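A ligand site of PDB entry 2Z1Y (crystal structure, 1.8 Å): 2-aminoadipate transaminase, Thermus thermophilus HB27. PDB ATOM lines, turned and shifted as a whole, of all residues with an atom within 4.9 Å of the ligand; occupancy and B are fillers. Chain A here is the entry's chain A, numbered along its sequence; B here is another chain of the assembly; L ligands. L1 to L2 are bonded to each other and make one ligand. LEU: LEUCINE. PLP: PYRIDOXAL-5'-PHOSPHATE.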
ATOM      1  N   ILE A  22     -20.368  13.293  13.613  1.00  0.00           N
ATOM      2  CA  ILE A  22     -20.145  12.375  12.488  1.00  0.00           C
ATOM      3  C   ILE A  22     -21.278  12.494  11.466  1.00  0.00           C
ATOM      4  O   ILE A  22     -21.002  12.654  10.271  1.00  0.00           O
ATOM      5  CB  ILE A  22     -19.956  10.943  13.004  1.00  0.00           C
ATOM      6  CG1 ILE A  22     -18.567  10.736  13.634  1.00  0.00           C
ATOM      7  CG2 ILE A  22     -20.200   9.878  11.914  1.00  0.00           C
ATOM      8  CD1 ILE A  22     -18.527   9.531  14.576  1.00  0.00           C
ATOM      9  N   LEU A  25     -21.151  15.775   9.493  1.00  0.00           N
ATOM     10  CA  LEU A  25     -20.052  15.845   8.543  1.00  0.00           C
ATOM     11  C   LEU A  25     -20.380  15.005   7.307  1.00  0.00           C
ATOM     12  O   LEU A  25     -19.973  15.337   6.194  1.00  0.00           O
ATOM     13  CB  LEU A  25     -18.717  15.389   9.136  1.00  0.00           C
ATOM     14  CG  LEU A  25     -18.121  16.227  10.274  1.00  0.00           C
ATOM     15  CD1 LEU A  25     -16.895  15.596  10.784  1.00  0.00           C
ATOM     16  CD2 LEU A  25     -17.864  17.657   9.897  1.00  0.00           C
ATOM     17  N   LEU A  26     -21.176  13.912   7.491  1.00  0.00           N
ATOM     18  CA  LEU A  26     -21.389  13.021   6.366  1.00  0.00           C
ATOM     19  C   LEU A  26     -22.556  13.423   5.492  1.00  0.00           C
ATOM     20  O   LEU A  26     -22.715  12.814   4.423  1.00  0.00           O
ATOM     21  CB  LEU A  26     -21.527  11.609   6.929  1.00  0.00           C
ATOM     22  CG  LEU A  26     -20.218  11.014   7.444  1.00  0.00           C
ATOM     23  CD1 LEU A  26     -20.562   9.704   8.235  1.00  0.00           C
ATOM     24  CD2 LEU A  26     -19.195  10.688   6.408  1.00  0.00           C
ATOM     25  N   ALA A  38     -14.796  20.908   6.097  1.00  0.00           N
ATOM     26  CA  ALA A  38     -15.325  20.264   7.300  1.00  0.00           C
ATOM     27  C   ALA A  38     -14.785  18.843   7.413  1.00  0.00           C
ATOM     28  O   ALA A  38     -13.726  18.601   7.915  1.00  0.00           O
ATOM     29  CB  ALA A  38     -16.812  20.336   7.225  1.00  0.00           C
ATOM     30  N   GLY A  39     -15.485  17.859   6.842  1.00  0.00           N
ATOM     31  CA  GLY A  39     -15.062  16.488   6.974  1.00  0.00           C
ATOM     32  C   GLY A  39     -13.759  16.230   6.286  1.00  0.00           C
ATOM     33  O   GLY A  39     -13.415  16.865   5.280  1.00  0.00           O
ATOM     34  N   GLY A  40     -13.043  15.281   6.827  1.00  0.00           N
ATOM     35  CA  GLY A  40     -11.798  14.817   6.269  1.00  0.00           C
ATOM     36  C   GLY A  40     -12.024  13.916   5.055  1.00  0.00           C
ATOM     37  O   GLY A  40     -11.629  12.758   5.070  1.00  0.00           O
ATOM     38  N   LEU A  41     -12.632  14.481   4.001  1.00  0.00           N
ATOM     39  CA  LEU A  41     -13.015  13.693   2.822  1.00  0.00           C
ATOM     40  C   LEU A  41     -11.863  13.681   1.837  1.00  0.00           C
ATOM     41  O   LEU A  41     -11.388  14.724   1.426  1.00  0.00           O
ATOM     42  CB  LEU A  41     -14.277  14.284   2.197  1.00  0.00           C
ATOM     43  CG  LEU A  41     -15.619  13.719   2.683  1.00  0.00           C
ATOM     44  CD1 LEU A  41     -15.958  14.031   4.152  1.00  0.00           C
ATOM     45  CD2 LEU A  41     -16.715  14.268   1.815  1.00  0.00           C
ATOM     46  N   GLY A  99     -14.171  -0.178   7.953  1.00  0.00           N
ATOM     47  CA  GLY A  99     -13.522   1.049   8.325  1.00  0.00           C
ATOM     48  C   GLY A  99     -12.821   0.930   9.670  1.00  0.00           C
ATOM     49  O   GLY A  99     -13.129   0.075  10.523  1.00  0.00           O
ATOM     50  N   SER A 100     -11.840   1.785   9.903  1.00  0.00           N
ATOM     51  CA  SER A 100     -11.169   1.759  11.201  1.00  0.00           C
ATOM     52  C   SER A 100     -12.091   2.317  12.285  1.00  0.00           C
ATOM     53  O   SER A 100     -11.855   2.121  13.479  1.00  0.00           O
ATOM     54  CB  SER A 100      -9.714   2.394  11.067  1.00  0.00           C
ATOM     55  OG  SER A 100      -9.907   3.782  10.817  1.00  0.00           O
ATOM     56  N   GLN A 101     -13.150   3.008  11.906  1.00  0.00           N
ATOM     57  CA  GLN A 101     -14.134   3.405  12.894  1.00  0.00           C
ATOM     58  C   GLN A 101     -14.741   2.156  13.597  1.00  0.00           C
ATOM     59  O   GLN A 101     -14.891   2.111  14.850  1.00  0.00           O
ATOM     60  CB  GLN A 101     -15.315   4.191  12.320  1.00  0.00           C
ATOM     61  CG  GLN A 101     -16.329   4.727  13.328  1.00  0.00           C
ATOM     62  CD  GLN A 101     -15.721   5.673  14.316  1.00  0.00           C
ATOM     63  OE1 GLN A 101     -14.905   6.486  13.945  1.00  0.00           O
ATOM     64  NE2 GLN A 101     -16.106   5.507  15.596  1.00  0.00           N
ATOM     65  N   LEU A 104     -12.283   0.939  16.179  1.00  0.00           N
ATOM     66  CA  LEU A 104     -12.381   1.703  17.414  1.00  0.00           C
ATOM     67  C   LEU A 104     -13.549   1.220  18.290  1.00  0.00           C
ATOM     68  O   LEU A 104     -13.422   1.078  19.513  1.00  0.00           O
ATOM     69  CB  LEU A 104     -12.539   3.199  17.053  1.00  0.00           C
ATOM     70  CG  LEU A 104     -11.312   3.840  16.383  1.00  0.00           C
ATOM     71  CD1 LEU A 104     -11.596   5.184  15.757  1.00  0.00           C
ATOM     72  CD2 LEU A 104     -10.135   3.980  17.322  1.00  0.00           C
ATOM     73  N   TYR A 125      -9.236  12.461  18.117  1.00  0.00           N
ATOM     74  CA  TYR A 125     -10.235  12.232  17.090  1.00  0.00           C
ATOM     75  C   TYR A 125     -11.645  12.050  17.647  1.00  0.00           C
ATOM     76  O   TYR A 125     -11.861  11.201  18.487  1.00  0.00           O
ATOM     77  CB  TYR A 125      -9.755  10.997  16.296  1.00  0.00           C
ATOM     78  CG  TYR A 125     -10.749  10.438  15.306  1.00  0.00           C
ATOM     79  CD1 TYR A 125     -11.365  11.262  14.382  1.00  0.00           C
ATOM     80  CD2 TYR A 125     -11.040   9.081  15.257  1.00  0.00           C
ATOM     81  CE1 TYR A 125     -12.349  10.768  13.537  1.00  0.00           C
ATOM     82  CE2 TYR A 125     -11.985   8.555  14.393  1.00  0.00           C
ATOM     83  CZ  TYR A 125     -12.630   9.417  13.517  1.00  0.00           C
ATOM     84  OH  TYR A 125     -13.600   8.920  12.722  1.00  0.00           O
ATOM     85  N   MET A 126     -12.603  12.835  17.137  1.00  0.00           N
ATOM     86  CA  MET A 126     -13.971  12.819  17.638  1.00  0.00           C
ATOM     87  C   MET A 126     -14.613  11.432  17.481  1.00  0.00           C
ATOM     88  O   MET A 126     -15.428  11.051  18.308  1.00  0.00           O
ATOM     89  CB  MET A 126     -14.839  13.914  17.010  1.00  0.00           C
ATOM     90  CG  MET A 126     -15.589  13.543  15.746  1.00  0.00           C
ATOM     91  SD  MET A 126     -14.385  13.722  14.443  1.00  0.00           S
ATOM     92  CE  MET A 126     -15.437  12.898  13.236  1.00  0.00           C
ATOM     93  N   TYR A 167      -4.843   5.889  23.630  1.00  0.00           N
ATOM     94  CA  TYR A 167      -5.192   6.002  22.205  1.00  0.00           C
ATOM     95  C   TYR A 167      -4.379   7.148  21.675  1.00  0.00           C
ATOM     96  O   TYR A 167      -4.518   8.274  22.177  1.00  0.00           O
ATOM     97  CB  TYR A 167      -6.726   6.253  22.046  1.00  0.00           C
ATOM     98  CG  TYR A 167      -7.146   6.651  20.650  1.00  0.00           C
ATOM     99  CD1 TYR A 167      -7.153   5.716  19.643  1.00  0.00           C
ATOM    100  CD2 TYR A 167      -7.382   7.988  20.304  1.00  0.00           C
ATOM    101  CE1 TYR A 167      -7.490   6.063  18.359  1.00  0.00           C
ATOM    102  CE2 TYR A 167      -7.719   8.336  19.020  1.00  0.00           C
ATOM    103  CZ  TYR A 167      -7.739   7.377  18.036  1.00  0.00           C
ATOM    104  OH  TYR A 167      -8.078   7.735  16.761  1.00  0.00           O
ATOM    105  N   ILE A 169      -2.475   8.973  17.896  1.00  0.00           N
ATOM    106  CA  ILE A 169      -2.389   9.131  16.445  1.00  0.00           C
ATOM    107  C   ILE A 169      -1.055   9.838  16.218  1.00  0.00           C
ATOM    108  O   ILE A 169      -0.946  11.076  16.102  1.00  0.00           O
ATOM    109  CB  ILE A 169      -3.579   9.946  15.869  1.00  0.00           C
ATOM    110  CG1 ILE A 169      -4.932   9.406  16.303  1.00  0.00           C
ATOM    111  CG2 ILE A 169      -3.533  10.014  14.346  1.00  0.00           C
ATOM    112  CD1 ILE A 169      -6.019  10.454  16.196  1.00  0.00           C
ATOM    113  N   ASN A 174      -5.387  13.669  14.114  1.00  0.00           N
ATOM    114  CA  ASN A 174      -6.711  14.309  13.978  1.00  0.00           C
ATOM    115  C   ASN A 174      -7.120  14.844  15.350  1.00  0.00           C
ATOM    116  O   ASN A 174      -7.356  14.035  16.247  1.00  0.00           O
ATOM    117  CB  ASN A 174      -7.705  13.302  13.437  1.00  0.00           C
ATOM    118  CG  ASN A 174      -9.042  13.865  13.026  1.00  0.00           C
ATOM    119  OD1 ASN A 174      -9.367  15.028  13.360  1.00  0.00           O
ATOM    120  ND2 ASN A 174      -9.815  13.066  12.291  1.00  0.00           N
ATOM    121  N   ASP A 202      -3.458   4.587  16.070  1.00  0.00           N
ATOM    122  CA  ASP A 202      -4.292   4.837  14.918  1.00  0.00           C
ATOM    123  C   ASP A 202      -3.449   5.501  13.835  1.00  0.00           C
ATOM    124  O   ASP A 202      -3.091   6.641  13.941  1.00  0.00           O
ATOM    125  CB  ASP A 202      -5.554   5.608  15.301  1.00  0.00           C
ATOM    126  CG  ASP A 202      -6.551   5.857  14.214  1.00  0.00           C
ATOM    127  OD1 ASP A 202      -6.179   5.689  13.003  1.00  0.00           O
ATOM    128  OD2 ASP A 202      -7.721   6.277  14.583  1.00  0.00           O
ATOM    129  N   ALA A 204      -4.289   6.134  10.544  1.00  0.00           N
ATOM    130  CA  ALA A 204      -5.030   6.481   9.331  1.00  0.00           C
ATOM    131  C   ALA A 204      -4.260   7.337   8.325  1.00  0.00           C
ATOM    132  O   ALA A 204      -4.475   7.140   7.112  1.00  0.00           O
ATOM    133  CB  ALA A 204      -6.305   7.227   9.717  1.00  0.00           C
ATOM    134  N   TYR A 205      -3.342   8.203   8.819  1.00  0.00           N
ATOM    135  CA  TYR A 205      -2.635   9.156   7.957  1.00  0.00           C
ATOM    136  C   TYR A 205      -1.187   8.735   7.721  1.00  0.00           C
ATOM    137  O   TYR A 205      -0.349   9.525   7.240  1.00  0.00           O
ATOM    138  CB  TYR A 205      -2.784  10.579   8.546  1.00  0.00           C
ATOM    139  CG  TYR A 205      -4.236  10.961   8.695  1.00  0.00           C
ATOM    140  CD1 TYR A 205      -5.022  11.347   7.621  1.00  0.00           C
ATOM    141  CD2 TYR A 205      -4.844  10.946   9.948  1.00  0.00           C
ATOM    142  CE1 TYR A 205      -6.354  11.609   7.788  1.00  0.00           C
ATOM    143  CE2 TYR A 205      -6.169  11.222  10.123  1.00  0.00           C
ATOM    144  CZ  TYR A 205      -6.958  11.543   9.035  1.00  0.00           C
ATOM    145  OH  TYR A 205      -8.309  11.771   9.234  1.00  0.00           O
ATOM    146  N   SER A 235      -6.126   1.933   7.622  1.00  0.00           N
ATOM    147  CA  SER A 235      -7.310   2.053   6.822  1.00  0.00           C
ATOM    148  C   SER A 235      -6.931   2.277   5.367  1.00  0.00           C
ATOM    149  O   SER A 235      -5.904   2.888   5.087  1.00  0.00           O
ATOM    150  CB  SER A 235      -8.127   3.174   7.314  1.00  0.00           C
ATOM    151  OG  SER A 235      -9.321   3.232   6.570  1.00  0.00           O
ATOM    152  N   SER A 237      -9.103   4.140   3.707  1.00  0.00           N
ATOM    153  CA  SER A 237      -9.954   5.281   3.476  1.00  0.00           C
ATOM    154  C   SER A 237      -9.180   6.486   2.912  1.00  0.00           C
ATOM    155  O   SER A 237      -9.681   7.137   2.009  1.00  0.00           O
ATOM    156  CB  SER A 237     -10.630   5.646   4.760  1.00  0.00           C
ATOM    157  OG  SER A 237     -11.635   4.692   5.118  1.00  0.00           O
ATOM    158  N   LYS A 238      -7.974   6.742   3.469  1.00  0.00           N
ATOM    159  CA  LYS A 238      -7.267   7.963   3.117  1.00  0.00           C
ATOM    160  C   LYS A 238      -6.400   7.774   1.874  1.00  0.00           C
ATOM    161  O   LYS A 238      -5.945   8.792   1.355  1.00  0.00           O
ATOM    162  CB  LYS A 238      -6.523   8.560   4.342  1.00  0.00           C
ATOM    163  CG  LYS A 238      -7.393   8.625   5.625  1.00  0.00           C
ATOM    164  CD  LYS A 238      -8.627   9.527   5.686  1.00  0.00           C
ATOM    165  CE  LYS A 238      -9.313   9.475   7.034  1.00  0.00           C
ATOM    166  NZ  LYS A 238     -10.312  10.574   7.122  1.00  0.00           N
ATOM    167  N   PRO A 242     -12.698   5.925   0.960  1.00  0.00           N
ATOM    168  CA  PRO A 242     -13.338   5.854   2.289  1.00  0.00           C
ATOM    169  C   PRO A 242     -14.702   5.188   2.202  1.00  0.00           C
ATOM    170  O   PRO A 242     -15.140   4.617   3.175  1.00  0.00           O
ATOM    171  CB  PRO A 242     -13.414   7.318   2.721  1.00  0.00           C
ATOM    172  CG  PRO A 242     -13.298   8.117   1.457  1.00  0.00           C
ATOM    173  CD  PRO A 242     -12.542   7.282   0.431  1.00  0.00           C
ATOM    174  N   ARG A 245     -15.394   1.405   2.937  1.00  0.00           N
ATOM    175  CA  ARG A 245     -15.308   0.938   4.329  1.00  0.00           C
ATOM    176  C   ARG A 245     -14.474  -0.340   4.472  1.00  0.00           C
ATOM    177  O   ARG A 245     -14.949  -1.414   4.886  1.00  0.00           O
ATOM    178  CB  ARG A 245     -16.690   0.781   4.963  1.00  0.00           C
ATOM    179  CG  ARG A 245     -17.750   1.799   4.617  1.00  0.00           C
ATOM    180  CD  ARG A 245     -17.494   3.235   5.032  1.00  0.00           C
ATOM    181  NE  ARG A 245     -17.176   3.332   6.461  1.00  0.00           N
ATOM    182  CZ  ARG A 245     -16.019   3.675   6.972  1.00  0.00           C
ATOM    183  NH1 ARG A 245     -15.005   4.022   6.152  1.00  0.00           N
ATOM    184  NH2 ARG A 245     -15.883   3.804   8.293  1.00  0.00           N
ATOM    185  N   ALA A 247     -10.769  -1.478   6.199  1.00  0.00           N
ATOM    186  CA  ALA A 247      -9.663  -1.147   7.034  1.00  0.00           C
ATOM    187  C   ALA A 247      -9.179  -2.367   7.814  1.00  0.00           C
ATOM    188  O   ALA A 247      -9.641  -3.498   7.560  1.00  0.00           O
ATOM    189  CB  ALA A 247     -10.132  -0.010   7.886  1.00  0.00           C
ATOM    190  N   PHE A 326      -5.250  18.050   7.773  1.00  0.00           N
ATOM    191  CA  PHE A 326      -5.866  19.108   8.566  1.00  0.00           C
ATOM    192  C   PHE A 326      -4.953  20.285   8.904  1.00  0.00           C
ATOM    193  O   PHE A 326      -3.787  20.102   9.208  1.00  0.00           O
ATOM    194  CB  PHE A 326      -6.419  18.601   9.878  1.00  0.00           C
ATOM    195  CG  PHE A 326      -7.351  17.407   9.673  1.00  0.00           C
ATOM    196  CD1 PHE A 326      -8.580  17.568   9.051  1.00  0.00           C
ATOM    197  CD2 PHE A 326      -7.008  16.152  10.139  1.00  0.00           C
ATOM    198  CE1 PHE A 326      -9.414  16.466   8.845  1.00  0.00           C
ATOM    199  CE2 PHE A 326      -7.866  15.066   9.962  1.00  0.00           C
ATOM    200  CZ  PHE A 326      -9.087  15.273   9.357  1.00  0.00           C
ATOM    201  N   ARG A 368     -11.127  22.949  13.253  1.00  0.00           N
ATOM    202  CA  ARG A 368     -10.335  22.185  12.321  1.00  0.00           C
ATOM    203  C   ARG A 368     -10.792  22.454  10.896  1.00  0.00           C
ATOM    204  O   ARG A 368     -11.996  22.553  10.600  1.00  0.00           O
ATOM    205  CB  ARG A 368     -10.613  20.698  12.582  1.00  0.00           C
ATOM    206  CG  ARG A 368      -9.643  19.736  11.932  1.00  0.00           C
ATOM    207  CD  ARG A 368     -10.152  18.290  11.987  1.00  0.00           C
ATOM    208  NE  ARG A 368     -11.325  18.043  11.137  1.00  0.00           N
ATOM    209  CZ  ARG A 368     -11.988  16.843  11.034  1.00  0.00           C
ATOM    210  NH1 ARG A 368     -11.658  15.782  11.756  1.00  0.00           N
ATOM    211  NH2 ARG A 368     -12.934  16.731  10.106  1.00  0.00           N
ATOM    212  N   TYR B  70     -16.899   9.156   1.361  1.00  0.00           N
ATOM    213  CA  TYR B  70     -17.720   9.178   2.557  1.00  0.00           C
ATOM    214  C   TYR B  70     -19.130   9.650   2.206  1.00  0.00           C
ATOM    215  O   TYR B  70     -19.318  10.556   1.353  1.00  0.00           O
ATOM    216  CB  TYR B  70     -17.112  10.067   3.621  1.00  0.00           C
ATOM    217  CG  TYR B  70     -15.948   9.523   4.426  1.00  0.00           C
ATOM    218  CD1 TYR B  70     -16.013   8.311   5.131  1.00  0.00           C
ATOM    219  CD2 TYR B  70     -14.771  10.217   4.506  1.00  0.00           C
ATOM    220  CE1 TYR B  70     -14.929   7.810   5.845  1.00  0.00           C
ATOM    221  CE2 TYR B  70     -13.703   9.777   5.275  1.00  0.00           C
ATOM    222  CZ  TYR B  70     -13.763   8.541   5.922  1.00  0.00           C
ATOM    223  OH  TYR B  70     -12.692   8.120   6.640  1.00  0.00           O
ATOM    224  N   LEU B 268     -19.437   4.626  10.844  1.00  0.00           N
ATOM    225  CA  LEU B 268     -19.666   5.875  10.124  1.00  0.00           C
ATOM    226  C   LEU B 268     -20.887   5.745   9.206  1.00  0.00           C
ATOM    227  O   LEU B 268     -21.810   6.496   9.370  1.00  0.00           O
ATOM    228  CB  LEU B 268     -18.462   6.442   9.391  1.00  0.00           C
ATOM    229  CG  LEU B 268     -17.161   6.598  10.194  1.00  0.00           C
ATOM    230  CD1 LEU B 268     -16.012   7.105   9.287  1.00  0.00           C
ATOM    231  CD2 LEU B 268     -17.343   7.562  11.354  1.00  0.00           C
HETATM  232  N   LEU L   1     -12.014  10.830   9.939  1.00  0.00           N
HETATM  233  CA  LEU L   1     -13.078  11.712   9.343  1.00  0.00           C
HETATM  234  C   LEU L   1     -12.924  13.130   9.914  1.00  0.00           C
HETATM  235  O   LEU L   1     -13.333  14.108   9.232  1.00  0.00           O
HETATM  236  CB  LEU L   1     -14.473  11.151   9.660  1.00  0.00           C
HETATM  237  CG  LEU L   1     -15.678  11.924   9.148  1.00  0.00           C
HETATM  238  CD1 LEU L   1     -15.747  12.031   7.635  1.00  0.00           C
HETATM  239  CD2 LEU L   1     -16.931  11.246   9.711  1.00  0.00           C
HETATM  240  OXT LEU L   1     -12.479  13.171  11.062  1.00  0.00           O
HETATM  241  N1  PLP L   2      -9.114   7.449  12.738  1.00  0.00           N
HETATM  242  C2  PLP L   2      -8.880   8.720  12.425  1.00  0.00           C
HETATM  243  C2A PLP L   2      -7.766   9.360  13.164  1.00  0.00           C
HETATM  244  C3  PLP L   2      -9.665   9.409  11.487  1.00  0.00           C
HETATM  245  O3  PLP L   2      -9.364  10.745  11.217  1.00  0.00           O
HETATM  246  C4  PLP L   2     -10.724   8.710  10.852  1.00  0.00           C
HETATM  247  C4A PLP L   2     -11.607   9.413   9.925  1.00  0.00           C
HETATM  248  C5  PLP L   2     -10.971   7.388  11.240  1.00  0.00           C
HETATM  249  C6  PLP L   2     -10.095   6.806  12.117  1.00  0.00           C
HETATM  250  C5A PLP L   2     -12.108   6.549  10.719  1.00  0.00           C
HETATM  251  O4P PLP L   2     -11.923   6.311   9.318  1.00  0.00           O
HETATM  252  P   PLP L   2     -12.390   4.964   8.570  1.00  0.00           P
HETATM  253  O1P PLP L   2     -11.207   4.086   8.459  1.00  0.00           O
HETATM  254  O2P PLP L   2     -13.474   4.294   9.409  1.00  0.00           O
HETATM  255  O3P PLP L   2     -12.795   5.526   7.199  1.00  0.00           O
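A nitrogen (N) of LEU L1 sits close to the side-chain amino group (NZ) of Lys 238.
The side-chain carboxylate (OD2) of Asp 202 lies within hydrogen-bond range of a nitrogen (N1) of PLP L2 (2.6 Å).
An oxygen (O2P) of PLP L2 is in hydrogen-bond range of the backbone NH (N) of Gln 101 (2.8 Å).
The side-chain amide nitrogen (ND2) of Asn 174 is in hydrogen-bond range of an oxygen (O3) of PLP L2, 2.6 Å away.
The side-chain hydroxyl (OG) of Ser 100 is in hydrogen-bond range of an oxygen (O1P) of PLP L2.
An oxygen (O1P) of PLP L2 sits at hydrogen-bond distance from the side-chain hydroxyl (OG) of Ser 235, 2.8 Å away.
The guanidinium group of Arg 245 lies within salt-bridge range of an oxygen (O2P) of PLP L2.
N of Ser 100 is in hydrogen-bond range of O1P of PLP L2 (2.8 Å).
An oxygen (O3P) of PLP L2 sits at hydrogen-bond distance from the side-chain hydroxyl (OG) of Ser 237, at 2.5 Å.
An oxygen (O3P) of PLP L2 lies within hydrogen-bond range of the side-chain hydroxyl (OH) of Tyr 70 of chain B, at 2.7 Å.
O of LEU L1 is in salt-bridge range of NH2 of Arg 368.
The backbone NH (N) of Gly 40 is in hydrogen-bond range of an oxygen (O) of LEU L1 (2.7 Å).
The side-chain hydroxyl (OH) of Tyr 205 lies within hydrogen-bond range of an oxygen (O3) of PLP L2.
Residues that only touch the ligand: Leu 26 (3.9 Å), Gly 39 (3.7 Å), Gly 99 (3.4 Å), Tyr 125 (3.4 Å), Met 126 (3.7 Å), Tyr 167 (3.96 Å), Ile 169 (3.7 Å) and Leu 268 of chain B (3.8 Å).
Hydrophobic or aromatic side chains within 4 Å of the ligand: Leu 26, Tyr 125, Met 126, Ile 169, Tyr 205, Tyr 70 of chain B and Leu 268 of chain B.
Along chain A the residues within 4 Å of the ligand span positions 26 to 368.
The nearest printed residue that does not touch the ligand is Leu 41 (4.02 Å).
The backbone NH of Ser 237 sits at hydrogen-bond distance from the side-chain hydroxyl of Ser 235 (3.0 Å).
OD1 of Asp 202 lies within hydrogen-bond range of N of Ala 204 (3.1 Å).
NZ of Lys 238 lies within hydrogen-bond range of OH of Tyr 205 (3.1 Å).
NH1 of Arg 368 sits at hydrogen-bond distance from OD1 of Asn 174 (2.9 Å).
The side-chain hydroxyl of Tyr 167 is in hydrogen-bond range of the side-chain carboxylate of Asp 202.
O of Gly 40 sits at hydrogen-bond distance from NZ of Lys 238, 3.3 Å away.
NH1 of Arg 245 is in hydrogen-bond range of O of Pro 242, at 3.0 Å.
The backbone carbonyl oxygen of Asn 174 is in hydrogen-bond range of the backbone NH of Tyr 125, at 3.1 Å.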
